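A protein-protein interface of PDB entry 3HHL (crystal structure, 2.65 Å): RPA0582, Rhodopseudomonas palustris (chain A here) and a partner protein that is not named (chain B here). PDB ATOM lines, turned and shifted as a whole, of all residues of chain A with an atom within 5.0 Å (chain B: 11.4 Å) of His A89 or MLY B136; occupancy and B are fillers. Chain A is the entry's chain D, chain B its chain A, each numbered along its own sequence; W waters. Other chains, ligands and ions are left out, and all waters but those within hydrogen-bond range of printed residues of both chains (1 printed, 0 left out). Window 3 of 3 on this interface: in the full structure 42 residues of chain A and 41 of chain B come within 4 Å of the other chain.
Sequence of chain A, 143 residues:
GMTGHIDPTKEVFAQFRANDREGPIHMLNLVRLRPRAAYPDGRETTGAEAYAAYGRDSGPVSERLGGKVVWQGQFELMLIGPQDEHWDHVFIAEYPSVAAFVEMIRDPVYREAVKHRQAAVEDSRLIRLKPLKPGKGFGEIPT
The backbone NH (N) of Leu B132 is in hydrogen-bond range of the backbone carbonyl oxygen (O) of Gln A72, 2.9 Å away.
NZ of MLY B136 sits close to the side-chain amide nitrogen (NE2) of Gln A72, 3.5 Å away.
O of Phe A91 is in hydrogen-bond range of N of Asn A29, at 2.8 Å.
N of Val A31 lies within hydrogen-bond range of O of His A89, at 2.9 Å.
Pro B134 touches Val A69 (CB to O, 3.5 Å).
Gln A72 touches Pro B131 (O to C, 3.8 Å).
CA of Pro B134 touches OE1 of Gln A72 (3.8 Å).
His A89 touches MLY B136.
CD2 of Leu B129 touches CB of Val A90 (3.6 Å).
CD1 of Phe A91 touches CH1 of MLY B136 (3.5 Å).
Printed residues of chain B within 4 Å of His A89: MLY B136.
Of chain A, only Gln A72 (3.3 Å), His A89 (3.97 Å) and Phe A91 (3.5 Å) come within 4 Å of MLY B136.
No residue of chain B comes within 4 Å of Leu A30.
No residue of chain B comes within 4 Å of Val A31.
No residue of chain B comes within 4 Å of Tyr A51.
No residue of chain B comes within 4 Å of Asp A88.
Of chain B, only Leu B129 comes within 4 Å of Val A90.
Phe A91 touches just one residue of chain B: MLY B136.
Of the printed residues of chain A, Leu B132 touches Gln A72 (2.9 Å).
Printed residues of chain B within 4 Å of Val A69: Pro B134 (3.5 Å).
Of the printed residues of chain A, Pro B134 touches Val A69 and Gln A72.
Of the printed residues of chain A, Pro B131 touches Gln A72 (3.8 Å).
The nearest residue of chain B that does not touch His A89 is Leu B129 (6.5 Å).
The nearest residue of chain A that does not touch MLY B136 is Tyr A51 (4.3 Å).
Of the 12 printed residues of chain A, 5 touch a printed residue of chain B.
Hydrophobic or aromatic side chains of chain A that line the printed part of chain B: Val A69, His A89, Val A90 and Phe A91.
Among the printed residues, no Asp or Glu carboxylate lies within 4 Å of a Lys or Arg side-chain nitrogen of the other chain.
Water W1 bridges the backbone carbonyl oxygen (O) of Leu B132 (2.7 Å) and the backbone NH (N) of Gln A72 (2.8 Å).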
ATOM      1  N   ASN A  29     -17.577 -36.210  20.183  1.00  0.00           N
ATOM      2  CA  ASN A  29     -18.912 -35.662  19.954  1.00  0.00           C
ATOM      3  C   ASN A  29     -18.814 -34.222  19.413  1.00  0.00           C
ATOM      4  O   ASN A  29     -18.180 -33.360  20.042  1.00  0.00           O
ATOM      5  CB  ASN A  29     -19.697 -35.603  21.276  1.00  0.00           C
ATOM      6  CG  ASN A  29     -20.201 -36.943  21.744  1.00  0.00           C
ATOM      7  OD1 ASN A  29     -21.386 -37.204  21.660  1.00  0.00           O
ATOM      8  ND2 ASN A  29     -19.318 -37.782  22.279  1.00  0.00           N
ATOM      9  N   LEU A  30     -19.460 -33.940  18.289  1.00  0.00           N
ATOM     10  CA  LEU A  30     -19.631 -32.567  17.828  1.00  0.00           C
ATOM     11  C   LEU A  30     -21.147 -32.263  17.835  1.00  0.00           C
ATOM     12  O   LEU A  30     -21.888 -32.864  17.094  1.00  0.00           O
ATOM     13  CB  LEU A  30     -19.066 -32.427  16.428  1.00  0.00           C
ATOM     14  CG  LEU A  30     -17.634 -32.944  16.228  1.00  0.00           C
ATOM     15  CD1 LEU A  30     -17.285 -32.906  14.762  1.00  0.00           C
ATOM     16  CD2 LEU A  30     -16.574 -32.150  17.045  1.00  0.00           C
ATOM     17  N   VAL A  31     -21.622 -31.357  18.677  1.00  0.00           N
ATOM     18  CA  VAL A  31     -23.055 -31.166  18.810  1.00  0.00           C
ATOM     19  C   VAL A  31     -23.518 -29.741  18.517  1.00  0.00           C
ATOM     20  O   VAL A  31     -23.060 -28.811  19.202  1.00  0.00           O
ATOM     21  CB  VAL A  31     -23.519 -31.475  20.245  1.00  0.00           C
ATOM     22  CG1 VAL A  31     -25.045 -31.477  20.274  1.00  0.00           C
ATOM     23  CG2 VAL A  31     -22.945 -32.793  20.754  1.00  0.00           C
ATOM     24  N   LEU A  33     -26.740 -27.460  18.788  1.00  0.00           N
ATOM     25  CA  LEU A  33     -28.024 -27.510  19.471  1.00  0.00           C
ATOM     26  C   LEU A  33     -29.070 -26.660  18.728  1.00  0.00           C
ATOM     27  O   LEU A  33     -28.740 -25.640  18.133  1.00  0.00           O
ATOM     28  CB  LEU A  33     -27.892 -27.013  20.906  1.00  0.00           C
ATOM     29  CG  LEU A  33     -27.067 -27.811  21.917  1.00  0.00           C
ATOM     30  CD1 LEU A  33     -26.936 -26.997  23.191  1.00  0.00           C
ATOM     31  CD2 LEU A  33     -27.682 -29.167  22.163  1.00  0.00           C
ATOM     32  N   TYR A  51     -30.535 -30.324  26.353  1.00  0.00           N
ATOM     33  CA  TYR A  51     -29.285 -31.043  26.361  1.00  0.00           C
ATOM     34  C   TYR A  51     -28.803 -31.198  27.809  1.00  0.00           C
ATOM     35  O   TYR A  51     -28.332 -32.250  28.187  1.00  0.00           O
ATOM     36  CB  TYR A  51     -28.248 -30.370  25.448  1.00  0.00           C
ATOM     37  CG  TYR A  51     -27.087 -31.274  25.137  1.00  0.00           C
ATOM     38  CD1 TYR A  51     -25.910 -31.201  25.854  1.00  0.00           C
ATOM     39  CD2 TYR A  51     -27.169 -32.234  24.139  1.00  0.00           C
ATOM     40  CE1 TYR A  51     -24.857 -32.079  25.596  1.00  0.00           C
ATOM     41  CE2 TYR A  51     -26.104 -33.091  23.864  1.00  0.00           C
ATOM     42  CZ  TYR A  51     -24.966 -33.004  24.592  1.00  0.00           C
ATOM     43  OH  TYR A  51     -23.930 -33.858  24.340  1.00  0.00           O
ATOM     44  N   VAL A  69     -15.728 -38.104  30.680  1.00  0.00           N
ATOM     45  CA  VAL A  69     -15.344 -37.115  29.704  1.00  0.00           C
ATOM     46  C   VAL A  69     -13.891 -36.867  29.927  1.00  0.00           C
ATOM     47  O   VAL A  69     -13.529 -36.379  30.969  1.00  0.00           O
ATOM     48  CB  VAL A  69     -16.121 -35.791  29.866  1.00  0.00           C
ATOM     49  CG1 VAL A  69     -15.456 -34.695  29.042  1.00  0.00           C
ATOM     50  CG2 VAL A  69     -17.552 -35.977  29.378  1.00  0.00           C
ATOM     51  N   GLN A  72     -12.593 -31.759  26.731  1.00  0.00           N
ATOM     52  CA  GLN A  72     -13.707 -30.910  26.366  1.00  0.00           C
ATOM     53  C   GLN A  72     -13.193 -29.538  25.966  1.00  0.00           C
ATOM     54  O   GLN A  72     -12.279 -29.018  26.596  1.00  0.00           O
ATOM     55  CB  GLN A  72     -14.634 -30.737  27.567  1.00  0.00           C
ATOM     56  CG  GLN A  72     -15.938 -30.074  27.168  1.00  0.00           C
ATOM     57  CD  GLN A  72     -17.020 -30.192  28.237  1.00  0.00           C
ATOM     58  OE1 GLN A  72     -16.762 -30.673  29.352  1.00  0.00           O
ATOM     59  NE2 GLN A  72     -18.238 -29.781  27.888  1.00  0.00           N
ATOM     60  N   TRP A  87     -20.232 -25.732  16.220  1.00  0.00           N
ATOM     61  CA  TRP A  87     -20.634 -26.708  17.188  1.00  0.00           C
ATOM     62  C   TRP A  87     -20.735 -26.025  18.520  1.00  0.00           C
ATOM     63  O   TRP A  87     -19.971 -25.104  18.802  1.00  0.00           O
ATOM     64  CB  TRP A  87     -19.602 -27.802  17.215  1.00  0.00           C
ATOM     65  CG  TRP A  87     -19.416 -28.431  15.889  1.00  0.00           C
ATOM     66  CD1 TRP A  87     -18.318 -28.362  15.112  1.00  0.00           C
ATOM     67  CD2 TRP A  87     -20.351 -29.238  15.183  1.00  0.00           C
ATOM     68  NE1 TRP A  87     -18.491 -29.091  13.960  1.00  0.00           N
ATOM     69  CE2 TRP A  87     -19.733 -29.646  13.984  1.00  0.00           C
ATOM     70  CE3 TRP A  87     -21.645 -29.677  15.455  1.00  0.00           C
ATOM     71  CZ2 TRP A  87     -20.371 -30.430  13.048  1.00  0.00           C
ATOM     72  CZ3 TRP A  87     -22.278 -30.474  14.525  1.00  0.00           C
ATOM     73  CH2 TRP A  87     -21.648 -30.836  13.332  1.00  0.00           C
ATOM     74  N   ASP A  88     -21.682 -26.471  19.334  1.00  0.00           N
ATOM     75  CA  ASP A  88     -21.953 -25.865  20.639  1.00  0.00           C
ATOM     76  C   ASP A  88     -21.268 -26.665  21.737  1.00  0.00           C
ATOM     77  O   ASP A  88     -20.840 -26.104  22.737  1.00  0.00           O
ATOM     78  CB  ASP A  88     -23.469 -25.848  20.876  1.00  0.00           C
ATOM     79  CG  ASP A  88     -24.177 -24.873  19.989  1.00  0.00           C
ATOM     80  OD1 ASP A  88     -23.850 -23.669  20.080  1.00  0.00           O
ATOM     81  OD2 ASP A  88     -25.056 -25.291  19.217  1.00  0.00           O
ATOM     82  N   HIS A  89     -21.222 -27.984  21.568  1.00  0.00           N
ATOM     83  CA  HIS A  89     -20.536 -28.832  22.480  1.00  0.00           C
ATOM     84  C   HIS A  89     -19.564 -29.670  21.699  1.00  0.00           C
ATOM     85  O   HIS A  89     -19.918 -30.240  20.677  1.00  0.00           O
ATOM     86  CB  HIS A  89     -21.521 -29.691  23.257  1.00  0.00           C
ATOM     87  CG  HIS A  89     -22.368 -28.896  24.192  1.00  0.00           C
ATOM     88  ND1 HIS A  89     -21.832 -27.997  25.091  1.00  0.00           N
ATOM     89  CD2 HIS A  89     -23.710 -28.841  24.365  1.00  0.00           C
ATOM     90  CE1 HIS A  89     -22.806 -27.416  25.772  1.00  0.00           C
ATOM     91  NE2 HIS A  89     -23.956 -27.896  25.339  1.00  0.00           N
ATOM     92  N   VAL A  90     -18.326 -29.726  22.176  1.00  0.00           N
ATOM     93  CA  VAL A  90     -17.299 -30.545  21.567  1.00  0.00           C
ATOM     94  C   VAL A  90     -16.552 -31.236  22.683  1.00  0.00           C
ATOM     95  O   VAL A  90     -15.972 -30.572  23.523  1.00  0.00           O
ATOM     96  CB  VAL A  90     -16.320 -29.697  20.711  1.00  0.00           C
ATOM     97  CG1 VAL A  90     -15.288 -30.577  19.974  1.00  0.00           C
ATOM     98  CG2 VAL A  90     -17.081 -28.905  19.711  1.00  0.00           C
ATOM     99  N   PHE A  91     -16.573 -32.566  22.709  1.00  0.00           N
ATOM    100  CA  PHE A  91     -15.889 -33.292  23.778  1.00  0.00           C
ATOM    101  C   PHE A  91     -15.574 -34.703  23.368  1.00  0.00           C
ATOM    102  O   PHE A  91     -16.149 -35.220  22.382  1.00  0.00           O
ATOM    103  CB  PHE A  91     -16.733 -33.335  25.067  1.00  0.00           C
ATOM    104  CG  PHE A  91     -18.048 -33.989  24.898  1.00  0.00           C
ATOM    105  CD1 PHE A  91     -19.111 -33.294  24.384  1.00  0.00           C
ATOM    106  CD2 PHE A  91     -18.225 -35.305  25.224  1.00  0.00           C
ATOM    107  CE1 PHE A  91     -20.380 -33.907  24.230  1.00  0.00           C
ATOM    108  CE2 PHE A  91     -19.478 -35.953  25.041  1.00  0.00           C
ATOM    109  CZ  PHE A  91     -20.556 -35.238  24.562  1.00  0.00           C
ATOM    110  N   LEU B  28      -8.397 -28.979  16.896  1.00  0.00           N
ATOM    111  CA  LEU B  28      -8.908 -30.299  16.492  1.00  0.00           C
ATOM    112  C   LEU B  28      -8.818 -30.428  14.984  1.00  0.00           C
ATOM    113  O   LEU B  28      -9.439 -29.660  14.257  1.00  0.00           O
ATOM    114  CB  LEU B  28     -10.324 -30.506  16.981  1.00  0.00           C
ATOM    115  CG  LEU B  28     -11.065 -31.774  16.584  1.00  0.00           C
ATOM    116  CD1 LEU B  28     -10.354 -33.060  16.981  1.00  0.00           C
ATOM    117  CD2 LEU B  28     -12.490 -31.698  17.192  1.00  0.00           C
ATOM    118  N   LEU B  30      -9.419 -32.785  11.649  1.00  0.00           N
ATOM    119  CA  LEU B  30      -9.989 -33.962  11.006  1.00  0.00           C
ATOM    120  C   LEU B  30      -9.459 -33.964   9.554  1.00  0.00           C
ATOM    121  O   LEU B  30      -9.731 -33.037   8.818  1.00  0.00           O
ATOM    122  CB  LEU B  30     -11.509 -33.932  11.019  1.00  0.00           C
ATOM    123  CG  LEU B  30     -12.180 -33.547  12.339  1.00  0.00           C
ATOM    124  CD1 LEU B  30     -13.681 -33.374  12.140  1.00  0.00           C
ATOM    125  CD2 LEU B  30     -11.869 -34.570  13.431  1.00  0.00           C
ATOM    126  N   ILE B  92      -5.672 -33.698  18.226  1.00  0.00           N
ATOM    127  CA  ILE B  92      -5.710 -32.362  18.807  1.00  0.00           C
ATOM    128  C   ILE B  92      -4.313 -31.885  19.075  1.00  0.00           C
ATOM    129  O   ILE B  92      -3.547 -32.565  19.715  1.00  0.00           O
ATOM    130  CB  ILE B  92      -6.541 -32.289  20.098  1.00  0.00           C
ATOM    131  CG1 ILE B  92      -8.035 -32.593  19.803  1.00  0.00           C
ATOM    132  CG2 ILE B  92      -6.336 -30.906  20.775  1.00  0.00           C
ATOM    133  CD1 ILE B  92      -8.862 -32.927  21.110  1.00  0.00           C
ATOM    134  N   ILE B 127     -10.647 -27.089  13.748  1.00  0.00           N
ATOM    135  CA  ILE B 127     -11.543 -26.423  14.676  1.00  0.00           C
ATOM    136  C   ILE B 127     -10.740 -25.878  15.823  1.00  0.00           C
ATOM    137  O   ILE B 127     -10.010 -26.622  16.458  1.00  0.00           O
ATOM    138  CB  ILE B 127     -12.556 -27.414  15.232  1.00  0.00           C
ATOM    139  CG1 ILE B 127     -13.198 -28.189  14.043  1.00  0.00           C
ATOM    140  CG2 ILE B 127     -13.554 -26.664  16.124  1.00  0.00           C
ATOM    141  CD1 ILE B 127     -14.339 -29.141  14.414  1.00  0.00           C
ATOM    142  N   ARG B 128     -10.869 -24.583  16.082  1.00  0.00           N
ATOM    143  CA  ARG B 128     -10.129 -23.978  17.160  1.00  0.00           C
ATOM    144  C   ARG B 128     -10.979 -24.042  18.400  1.00  0.00           C
ATOM    145  O   ARG B 128     -12.105 -23.582  18.347  1.00  0.00           O
ATOM    146  CB  ARG B 128      -9.812 -22.538  16.852  1.00  0.00           C
ATOM    147  CG  ARG B 128      -9.331 -21.789  18.056  1.00  0.00           C
ATOM    148  CD  ARG B 128      -9.223 -20.315  17.762  1.00  0.00           C
ATOM    149  NE  ARG B 128      -9.095 -19.516  18.965  1.00  0.00           N
ATOM    150  CZ  ARG B 128      -8.600 -18.292  19.024  1.00  0.00           C
ATOM    151  NH1 ARG B 128      -8.152 -17.692  17.958  1.00  0.00           N
ATOM    152  NH2 ARG B 128      -8.561 -17.648  20.179  1.00  0.00           N
ATOM    153  N   LEU B 129     -10.441 -24.577  19.506  1.00  0.00           N
ATOM    154  CA  LEU B 129     -11.174 -24.585  20.755  1.00  0.00           C
ATOM    155  C   LEU B 129     -10.384 -24.023  21.927  1.00  0.00           C
ATOM    156  O   LEU B 129      -9.178 -24.059  21.935  1.00  0.00           O
ATOM    157  CB  LEU B 129     -11.630 -25.983  21.068  1.00  0.00           C
ATOM    158  CG  LEU B 129     -12.366 -26.698  19.919  1.00  0.00           C
ATOM    159  CD1 LEU B 129     -11.421 -27.741  19.256  1.00  0.00           C
ATOM    160  CD2 LEU B 129     -13.648 -27.331  20.398  1.00  0.00           C
ATOM    161  N   MLZ B 130     -11.088 -23.470  22.901  1.00  0.00           N
ATOM    162  CA  MLZ B 130     -10.502 -23.184  24.195  1.00  0.00           C
ATOM    163  CB  MLZ B 130     -11.127 -21.974  24.812  1.00  0.00           C
ATOM    164  CG  MLZ B 130     -10.822 -21.817  26.287  1.00  0.00           C
ATOM    165  CD  MLZ B 130     -11.048 -20.473  26.645  1.00  0.00           C
ATOM    166  CE  MLZ B 130     -11.432 -20.271  27.974  1.00  0.00           C
ATOM    167  NZ  MLZ B 130     -12.477 -19.187  27.960  1.00  0.00           N
ATOM    168  CM  MLZ B 130     -12.164 -18.017  27.061  1.00  0.00           C
ATOM    169  C   MLZ B 130     -10.727 -24.407  25.095  1.00  0.00           C
ATOM    170  O   MLZ B 130     -11.845 -24.822  25.319  1.00  0.00           O
ATOM    171  N   PRO B 131      -9.663 -24.990  25.607  1.00  0.00           N
ATOM    172  CA  PRO B 131      -9.775 -26.110  26.558  1.00  0.00           C
ATOM    173  C   PRO B 131     -10.631 -25.781  27.765  1.00  0.00           C
ATOM    174  O   PRO B 131     -10.457 -24.736  28.339  1.00  0.00           O
ATOM    175  CB  PRO B 131      -8.335 -26.339  27.036  1.00  0.00           C
ATOM    176  CG  PRO B 131      -7.498 -25.650  26.102  1.00  0.00           C
ATOM    177  CD  PRO B 131      -8.284 -24.582  25.394  1.00  0.00           C
ATOM    178  N   LEU B 132     -11.513 -26.688  28.140  1.00  0.00           N
ATOM    179  CA  LEU B 132     -12.262 -26.578  29.374  1.00  0.00           C
ATOM    180  C   LEU B 132     -11.826 -27.646  30.386  1.00  0.00           C
ATOM    181  O   LEU B 132     -11.311 -28.683  30.001  1.00  0.00           O
ATOM    182  CB  LEU B 132     -13.744 -26.703  29.067  1.00  0.00           C
ATOM    183  CG  LEU B 132     -14.315 -25.716  28.051  1.00  0.00           C
ATOM    184  CD1 LEU B 132     -15.676 -26.122  27.602  1.00  0.00           C
ATOM    185  CD2 LEU B 132     -14.324 -24.310  28.638  1.00  0.00           C
ATOM    186  N   LYS B 133     -11.968 -27.364  31.680  1.00  0.00           N
ATOM    187  CA  LYS B 133     -11.915 -28.438  32.701  1.00  0.00           C
ATOM    188  C   LYS B 133     -13.099 -29.350  32.394  1.00  0.00           C
ATOM    189  O   LYS B 133     -14.229 -28.875  32.472  1.00  0.00           O
ATOM    190  CB  LYS B 133     -12.081 -27.907  34.148  1.00  0.00           C
ATOM    191  CG  LYS B 133     -10.759 -27.481  34.884  1.00  0.00           C
ATOM    192  CD  LYS B 133     -11.032 -26.786  36.260  1.00  0.00           C
ATOM    193  N   PRO B 134     -12.868 -30.650  32.067  1.00  0.00           N
ATOM    194  CA  PRO B 134     -14.010 -31.554  31.747  1.00  0.00           C
ATOM    195  C   PRO B 134     -15.079 -31.734  32.880  1.00  0.00           C
ATOM    196  O   PRO B 134     -15.232 -32.818  33.449  1.00  0.00           O
ATOM    197  CB  PRO B 134     -13.319 -32.885  31.409  1.00  0.00           C
ATOM    198  CG  PRO B 134     -11.822 -32.568  31.268  1.00  0.00           C
ATOM    199  CD  PRO B 134     -11.594 -31.399  32.152  1.00  0.00           C
ATOM    200  N   GLY B 135     -15.743 -30.622  33.224  1.00  0.00           N
ATOM    201  CA  GLY B 135     -17.036 -30.551  33.950  1.00  0.00           C
ATOM    202  C   GLY B 135     -17.808 -29.426  33.230  1.00  0.00           C
ATOM    203  O   GLY B 135     -17.337 -28.266  33.234  1.00  0.00           O
ATOM    204  N   MLY B 136     -18.958 -29.769  32.610  1.00  0.00           N
ATOM    205  CA  MLY B 136     -19.686 -28.922  31.584  1.00  0.00           C
ATOM    206  CB  MLY B 136     -21.203 -29.300  31.488  1.00  0.00           C
ATOM    207  CG  MLY B 136     -22.034 -28.857  30.254  1.00  0.00           C
ATOM    208  CD  MLY B 136     -21.620 -29.520  28.923  1.00  0.00           C
ATOM    209  CE  MLY B 136     -21.997 -31.015  28.844  1.00  0.00           C
ATOM    210  NZ  MLY B 136     -20.966 -31.896  28.269  1.00  0.00           N
ATOM    211  CH1 MLY B 136     -20.809 -31.588  26.861  1.00  0.00           C
ATOM    212  CH2 MLY B 136     -21.298 -33.321  28.433  1.00  0.00           C
ATOM    213  C   MLY B 136     -19.507 -27.384  31.715  1.00  0.00           C
ATOM    214  O   MLY B 136     -18.627 -26.770  31.078  1.00  0.00           O
HETATM  215  O   HOH W   1     -10.640 -30.751  28.482  1.00  0.00           O
